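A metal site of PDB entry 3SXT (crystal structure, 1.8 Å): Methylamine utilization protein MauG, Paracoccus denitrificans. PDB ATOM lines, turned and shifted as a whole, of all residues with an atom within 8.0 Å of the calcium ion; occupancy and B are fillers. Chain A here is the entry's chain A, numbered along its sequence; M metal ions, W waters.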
ATOM      1  N   ARG A  39      10.480  12.542  16.384  1.00  0.00           N
ATOM      2  CA  ARG A  39      10.215  11.420  15.433  1.00  0.00           C
ATOM      3  C   ARG A  39       8.959  11.682  14.586  1.00  0.00           C
ATOM      4  O   ARG A  39       8.053  10.817  14.432  1.00  0.00           O
ATOM      5  CB  ARG A  39      10.111  10.124  16.253  1.00  0.00           C
ATOM      6  CG  ARG A  39      10.263   8.844  15.412  1.00  0.00           C
ATOM      7  CD  ARG A  39       9.817   7.692  16.259  1.00  0.00           C
ATOM      8  NE  ARG A  39      10.279   6.431  15.608  1.00  0.00           N
ATOM      9  CZ  ARG A  39       9.562   5.669  14.796  1.00  0.00           C
ATOM     10  NH1 ARG A  39      10.139   4.574  14.287  1.00  0.00           N
ATOM     11  NH2 ARG A  39       8.301   5.958  14.476  1.00  0.00           N
ATOM     12  N   THR A  42       5.625  10.840  16.306  1.00  0.00           N
ATOM     13  CA  THR A  42       5.189   9.445  16.546  1.00  0.00           C
ATOM     14  C   THR A  42       5.978   8.873  17.704  1.00  0.00           C
ATOM     15  O   THR A  42       6.782   9.596  18.349  1.00  0.00           O
ATOM     16  CB  THR A  42       5.375   8.562  15.266  1.00  0.00           C
ATOM     17  OG1 THR A  42       6.766   8.492  14.990  1.00  0.00           O
ATOM     18  CG2 THR A  42       4.721   9.252  14.040  1.00  0.00           C
ATOM     19  N   ASP A  43       5.725   7.584  18.016  1.00  0.00           N
ATOM     20  CA  ASP A  43       6.191   6.989  19.277  1.00  0.00           C
ATOM     21  C   ASP A  43       7.471   6.124  19.099  1.00  0.00           C
ATOM     22  O   ASP A  43       7.422   5.060  18.427  1.00  0.00           O
ATOM     23  CB  ASP A  43       5.077   6.192  19.940  1.00  0.00           C
ATOM     24  CG  ASP A  43       5.422   5.811  21.444  1.00  0.00           C
ATOM     25  OD1 ASP A  43       4.527   5.247  22.122  1.00  0.00           O
ATOM     26  OD2 ASP A  43       6.547   6.092  21.893  1.00  0.00           O
ATOM     27  N   LEU A  51       7.320  -1.482  18.060  1.00  0.00           N
ATOM     28  CA  LEU A  51       6.802  -0.093  17.887  1.00  0.00           C
ATOM     29  C   LEU A  51       5.405  -0.045  17.267  1.00  0.00           C
ATOM     30  O   LEU A  51       4.922   1.030  16.886  1.00  0.00           O
ATOM     31  CB  LEU A  51       7.784   0.732  17.038  1.00  0.00           C
ATOM     32  CG  LEU A  51       8.746   1.587  17.916  1.00  0.00           C
ATOM     33  CD1 LEU A  51       9.550   0.653  18.698  1.00  0.00           C
ATOM     34  CD2 LEU A  51       9.678   2.424  17.046  1.00  0.00           C
ATOM     35  N   ALA A  52       4.741  -1.210  17.209  1.00  0.00           N
ATOM     36  CA  ALA A  52       3.398  -1.252  16.570  1.00  0.00           C
ATOM     37  C   ALA A  52       2.309  -0.440  17.291  1.00  0.00           C
ATOM     38  O   ALA A  52       1.502   0.216  16.639  1.00  0.00           O
ATOM     39  CB  ALA A  52       2.941  -2.669  16.334  1.00  0.00           C
ATOM     40  N   ASN A  66      -1.657   1.783  15.777  1.00  0.00           N
ATOM     41  CA  ASN A  66      -0.372   2.482  15.723  1.00  0.00           C
ATOM     42  C   ASN A  66      -0.550   4.016  15.921  1.00  0.00           C
ATOM     43  O   ASN A  66      -1.476   4.630  15.362  1.00  0.00           O
ATOM     44  CB  ASN A  66       0.250   2.115  14.377  1.00  0.00           C
ATOM     45  CG  ASN A  66       1.643   2.753  14.186  1.00  0.00           C
ATOM     46  OD1 ASN A  66       1.834   3.631  13.373  1.00  0.00           O
ATOM     47  ND2 ASN A  66       2.575   2.340  14.994  1.00  0.00           N
ATOM     48  N   THR A  67       0.332   4.655  16.696  1.00  0.00           N
ATOM     49  CA  THR A  67       0.253   6.119  16.921  1.00  0.00           C
ATOM     50  C   THR A  67       0.651   6.827  15.600  1.00  0.00           C
ATOM     51  O   THR A  67       1.799   6.623  15.109  1.00  0.00           O
ATOM     52  CB  THR A  67       1.180   6.491  18.038  1.00  0.00           C
ATOM     53  OG1 THR A  67       0.653   5.886  19.240  1.00  0.00           O
ATOM     54  CG2 THR A  67       1.298   8.023  18.169  1.00  0.00           C
ATOM     55  N   PRO A  68      -0.249   7.608  15.031  1.00  0.00           N
ATOM     56  CA  PRO A  68       0.039   8.314  13.795  1.00  0.00           C
ATOM     57  C   PRO A  68       0.741   9.643  14.027  1.00  0.00           C
ATOM     58  O   PRO A  68       0.652  10.213  15.068  1.00  0.00           O
ATOM     59  CB  PRO A  68      -1.337   8.578  13.214  1.00  0.00           C
ATOM     60  CG  PRO A  68      -2.192   8.707  14.353  1.00  0.00           C
ATOM     61  CD  PRO A  68      -1.648   7.781  15.429  1.00  0.00           C
ATOM     62  N   THR A  69       1.418  10.120  13.015  1.00  0.00           N
ATOM     63  CA  THR A  69       1.966  11.448  13.059  1.00  0.00           C
ATOM     64  C   THR A  69       0.897  12.539  13.232  1.00  0.00           C
ATOM     65  O   THR A  69      -0.266  12.371  12.807  1.00  0.00           O
ATOM     66  CB  THR A  69       2.728  11.737  11.757  1.00  0.00           C
ATOM     67  OG1 THR A  69       3.446  12.959  11.895  1.00  0.00           O
ATOM     68  CG2 THR A  69       1.753  11.810  10.532  1.00  0.00           C
ATOM     69  N   TRP A  93      -7.667   6.853  13.036  1.00  0.00           N
ATOM     70  CA  TRP A  93      -7.669   5.984  11.871  1.00  0.00           C
ATOM     71  C   TRP A  93      -9.114   5.652  11.415  1.00  0.00           C
ATOM     72  O   TRP A  93      -9.320   5.291  10.292  1.00  0.00           O
ATOM     73  CB  TRP A  93      -6.939   4.682  12.181  1.00  0.00           C
ATOM     74  CG  TRP A  93      -5.468   4.809  12.284  1.00  0.00           C
ATOM     75  CD1 TRP A  93      -4.751   4.957  13.430  1.00  0.00           C
ATOM     76  CD2 TRP A  93      -4.504   4.712  11.217  1.00  0.00           C
ATOM     77  NE1 TRP A  93      -3.414   4.953  13.167  1.00  0.00           N
ATOM     78  CE2 TRP A  93      -3.224   4.816  11.807  1.00  0.00           C
ATOM     79  CE3 TRP A  93      -4.614   4.544   9.796  1.00  0.00           C
ATOM     80  CZ2 TRP A  93      -2.030   4.758  11.061  1.00  0.00           C
ATOM     81  CZ3 TRP A  93      -3.448   4.504   9.049  1.00  0.00           C
ATOM     82  CH2 TRP A  93      -2.160   4.582   9.686  1.00  0.00           C
ATOM     83  N   ASN A 271       6.348  12.406   5.644  1.00  0.00           N
ATOM     84  CA  ASN A 271       7.239  11.855   6.662  1.00  0.00           C
ATOM     85  C   ASN A 271       7.116  10.322   6.793  1.00  0.00           C
ATOM     86  O   ASN A 271       7.630   9.730   7.773  1.00  0.00           O
ATOM     87  CB  ASN A 271       7.087  12.526   8.054  1.00  0.00           C
ATOM     88  CG  ASN A 271       7.551  13.967   8.034  1.00  0.00           C
ATOM     89  OD1 ASN A 271       8.618  14.235   7.478  1.00  0.00           O
ATOM     90  ND2 ASN A 271       6.708  14.902   8.561  1.00  0.00           N
ATOM     91  N   VAL A 272       6.516   9.672   5.776  1.00  0.00           N
ATOM     92  CA  VAL A 272       6.308   8.236   5.869  1.00  0.00           C
ATOM     93  C   VAL A 272       7.596   7.491   6.087  1.00  0.00           C
ATOM     94  O   VAL A 272       7.602   6.461   6.796  1.00  0.00           O
ATOM     95  CB  VAL A 272       5.542   7.666   4.650  1.00  0.00           C
ATOM     96  CG1 VAL A 272       6.345   7.677   3.292  1.00  0.00           C
ATOM     97  CG2 VAL A 272       5.108   6.265   4.948  1.00  0.00           C
ATOM     98  N   VAL A 274      10.099   8.002   7.958  1.00  0.00           N
ATOM     99  CA  VAL A 274      10.615   8.030   9.345  1.00  0.00           C
ATOM    100  C   VAL A 274       9.560   7.675  10.392  1.00  0.00           C
ATOM    101  O   VAL A 274       9.784   7.847  11.608  1.00  0.00           O
ATOM    102  CB  VAL A 274      11.209   9.461   9.654  1.00  0.00           C
ATOM    103  CG1 VAL A 274      12.219   9.782   8.546  1.00  0.00           C
ATOM    104  CG2 VAL A 274      10.171  10.559   9.649  1.00  0.00           C
ATOM    105  N   THR A 275       8.374   7.240   9.957  1.00  0.00           N
ATOM    106  CA  THR A 275       7.278   7.018  10.920  1.00  0.00           C
ATOM    107  C   THR A 275       6.834   5.519  10.948  1.00  0.00           C
ATOM    108  O   THR A 275       5.703   5.174  11.324  1.00  0.00           O
ATOM    109  CB  THR A 275       6.055   7.882  10.612  1.00  0.00           C
ATOM    110  OG1 THR A 275       5.605   7.569   9.304  1.00  0.00           O
ATOM    111  CG2 THR A 275       6.341   9.407  10.714  1.00  0.00           C
ATOM    112  N   GLY A 276       7.710   4.635  10.547  1.00  0.00           N
ATOM    113  CA  GLY A 276       7.441   3.182  10.697  1.00  0.00           C
ATOM    114  C   GLY A 276       7.190   2.814  12.170  1.00  0.00           C
ATOM    115  O   GLY A 276       7.583   3.533  13.061  1.00  0.00           O
ATOM    116  N   PRO A 277       6.592   1.639  12.430  1.00  0.00           N
ATOM    117  CA  PRO A 277       6.064   0.671  11.506  1.00  0.00           C
ATOM    118  C   PRO A 277       4.744   1.209  10.888  1.00  0.00           C
ATOM    119  O   PRO A 277       4.262   2.291  11.273  1.00  0.00           O
ATOM    120  CB  PRO A 277       5.786  -0.563  12.388  1.00  0.00           C
ATOM    121  CG  PRO A 277       5.482  -0.014  13.799  1.00  0.00           C
ATOM    122  CD  PRO A 277       6.438   1.247  13.853  1.00  0.00           C
ATOM    123  N   TYR A 278       4.158   0.462   9.953  1.00  0.00           N
ATOM    124  CA  TYR A 278       3.221   1.100   8.982  1.00  0.00           C
ATOM    125  C   TYR A 278       1.848   0.436   9.155  1.00  0.00           C
ATOM    126  O   TYR A 278       1.734  -0.685   9.710  1.00  0.00           O
ATOM    127  CB  TYR A 278       3.732   0.918   7.526  1.00  0.00           C
ATOM    128  CG  TYR A 278       4.994   1.684   7.366  1.00  0.00           C
ATOM    129  CD1 TYR A 278       6.244   1.039   7.384  1.00  0.00           C
ATOM    130  CD2 TYR A 278       4.971   3.107   7.400  1.00  0.00           C
ATOM    131  CE1 TYR A 278       7.444   1.801   7.295  1.00  0.00           C
ATOM    132  CE2 TYR A 278       6.172   3.854   7.336  1.00  0.00           C
ATOM    133  CZ  TYR A 278       7.370   3.201   7.312  1.00  0.00           C
ATOM    134  OH  TYR A 278       8.505   3.910   7.193  1.00  0.00           O
ATOM    135  N   MET A 279       0.826   1.109   8.643  1.00  0.00           N
ATOM    136  CA  MET A 279      -0.590   0.757   8.713  1.00  0.00           C
ATOM    137  C   MET A 279      -1.194   1.010  10.088  1.00  0.00           C
ATOM    138  O   MET A 279      -0.477   1.356  11.053  1.00  0.00           O
ATOM    139  CB  MET A 279      -0.872  -0.687   8.203  1.00  0.00           C
ATOM    140  CG  MET A 279      -0.184  -0.938   6.808  1.00  0.00           C
ATOM    141  SD  MET A 279      -0.848   0.166   5.536  1.00  0.00           S
ATOM    142  CE  MET A 279       0.164  -0.444   4.166  1.00  0.00           C
ATOM    143  N   HIS A 280      -2.534   0.847  10.164  1.00  0.00           N
ATOM    144  CA  HIS A 280      -3.302   1.249  11.332  1.00  0.00           C
ATOM    145  C   HIS A 280      -2.915   0.425  12.540  1.00  0.00           C
ATOM    146  O   HIS A 280      -3.140   0.853  13.642  1.00  0.00           O
ATOM    147  CB  HIS A 280      -4.855   1.162  11.068  1.00  0.00           C
ATOM    148  CG  HIS A 280      -5.333  -0.264  10.853  1.00  0.00           C
ATOM    149  ND1 HIS A 280      -5.583  -0.793   9.585  1.00  0.00           N
ATOM    150  CD2 HIS A 280      -5.548  -1.286  11.724  1.00  0.00           C
ATOM    151  CE1 HIS A 280      -5.912  -2.061   9.701  1.00  0.00           C
ATOM    152  NE2 HIS A 280      -5.912  -2.388  10.983  1.00  0.00           N
ATOM    153  N   ASN A 281      -2.324  -0.755  12.336  1.00  0.00           N
ATOM    154  CA  ASN A 281      -1.942  -1.658  13.428  1.00  0.00           C
ATOM    155  C   ASN A 281      -0.404  -1.863  13.454  1.00  0.00           C
ATOM    156  O   ASN A 281       0.116  -2.727  14.165  1.00  0.00           O
ATOM    157  CB  ASN A 281      -2.725  -2.968  13.328  1.00  0.00           C
ATOM    158  CG  ASN A 281      -2.516  -3.663  11.953  1.00  0.00           C
ATOM    159  OD1 ASN A 281      -1.621  -3.275  11.187  1.00  0.00           O
ATOM    160  ND2 ASN A 281      -3.337  -4.641  11.654  1.00  0.00           N
ATOM    161  N   GLY A 282       0.333  -1.046  12.715  1.00  0.00           N
ATOM    162  CA  GLY A 282       1.830  -1.174  12.744  1.00  0.00           C
ATOM    163  C   GLY A 282       2.367  -2.539  12.320  1.00  0.00           C
ATOM    164  O   GLY A 282       3.416  -2.963  12.765  1.00  0.00           O
ATOM    165  N   VAL A 283       1.643  -3.214  11.448  1.00  0.00           N
ATOM    166  CA  VAL A 283       2.005  -4.586  11.092  1.00  0.00           C
ATOM    167  C   VAL A 283       3.310  -4.708  10.315  1.00  0.00           C
ATOM    168  O   VAL A 283       3.974  -5.684  10.486  1.00  0.00           O
ATOM    169  CB  VAL A 283       0.790  -5.304  10.387  1.00  0.00           C
ATOM    170  CG1 VAL A 283       0.479  -4.661   9.052  1.00  0.00           C
ATOM    171  CG2 VAL A 283       1.026  -6.823  10.251  1.00  0.00           C
ATOM    172  N   PHE A 284       3.673  -3.727   9.472  1.00  0.00           N
ATOM    173  CA  PHE A 284       4.906  -3.864   8.699  1.00  0.00           C
ATOM    174  C   PHE A 284       5.988  -2.932   9.230  1.00  0.00           C
ATOM    175  O   PHE A 284       5.702  -1.727   9.410  1.00  0.00           O
ATOM    176  CB  PHE A 284       4.675  -3.508   7.209  1.00  0.00           C
ATOM    177  CG  PHE A 284       3.532  -4.244   6.593  1.00  0.00           C
ATOM    178  CD1 PHE A 284       3.387  -5.639   6.845  1.00  0.00           C
ATOM    179  CD2 PHE A 284       2.601  -3.553   5.774  1.00  0.00           C
ATOM    180  CE1 PHE A 284       2.311  -6.343   6.277  1.00  0.00           C
ATOM    181  CE2 PHE A 284       1.496  -4.239   5.206  1.00  0.00           C
ATOM    182  CZ  PHE A 284       1.372  -5.620   5.419  1.00  0.00           C
HETATM  183 CA    CA M   1       3.480   4.487  11.717  1.00  0.00          CA
HETATM  184  O   HOH W   1       1.424   3.772  10.583  1.00  0.00           O
HETATM  185  O   HOH W   2       2.894   6.619  12.636  1.00  0.00           O
HETATM  186  O   HOH W   3       3.551   5.575   9.715  1.00  0.00           O
HETATM  187  O   HOH W   4       4.778   4.298  13.926  1.00  0.00           O
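O of Val 272 is in hydrogen-bond range of OG1 of Thr 275, at 3.4 Å. OG1 of Thr 275 lies close to O of Asn 271 (3.3 Å). The backbone carbonyl oxygen (O) of Asn 66 lies within hydrogen-bond range of the indole nitrogen (NE1) of Trp 93, at 2.9 Å. O of Leu 51 sits at hydrogen-bond distance from ND2 of Asn 66, 3.3 Å away. The side-chain amide nitrogen (ND2) of Asn 66 lies within hydrogen-bond range of the backbone carbonyl oxygen (O) of Ala 52 (2.9 Å). The backbone NH (N) of Asn 66 lies within hydrogen-bond range of the backbone carbonyl oxygen (O) of His 280 (2.8 Å).
The nearest printed residue that does not touch the calcium ion is Gly 276 (4.1 Å).
The calcium ion is bound by water W3 (2.3 Å), O of Thr 275 (2.4 Å), O of Pro 277 (2.4 Å), water W2 (2.4 Å), water W1 (2.5 Å), OD1 of Asn 66 (2.5 Å) and water W4 (2.6 Å). The calcium ion has seven donor atoms within binding distance.
Water W4 lies within hydrogen-bond range of O of Gly 276 (3.0 Å) and ND2 of Asn 66 (3.1 Å).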
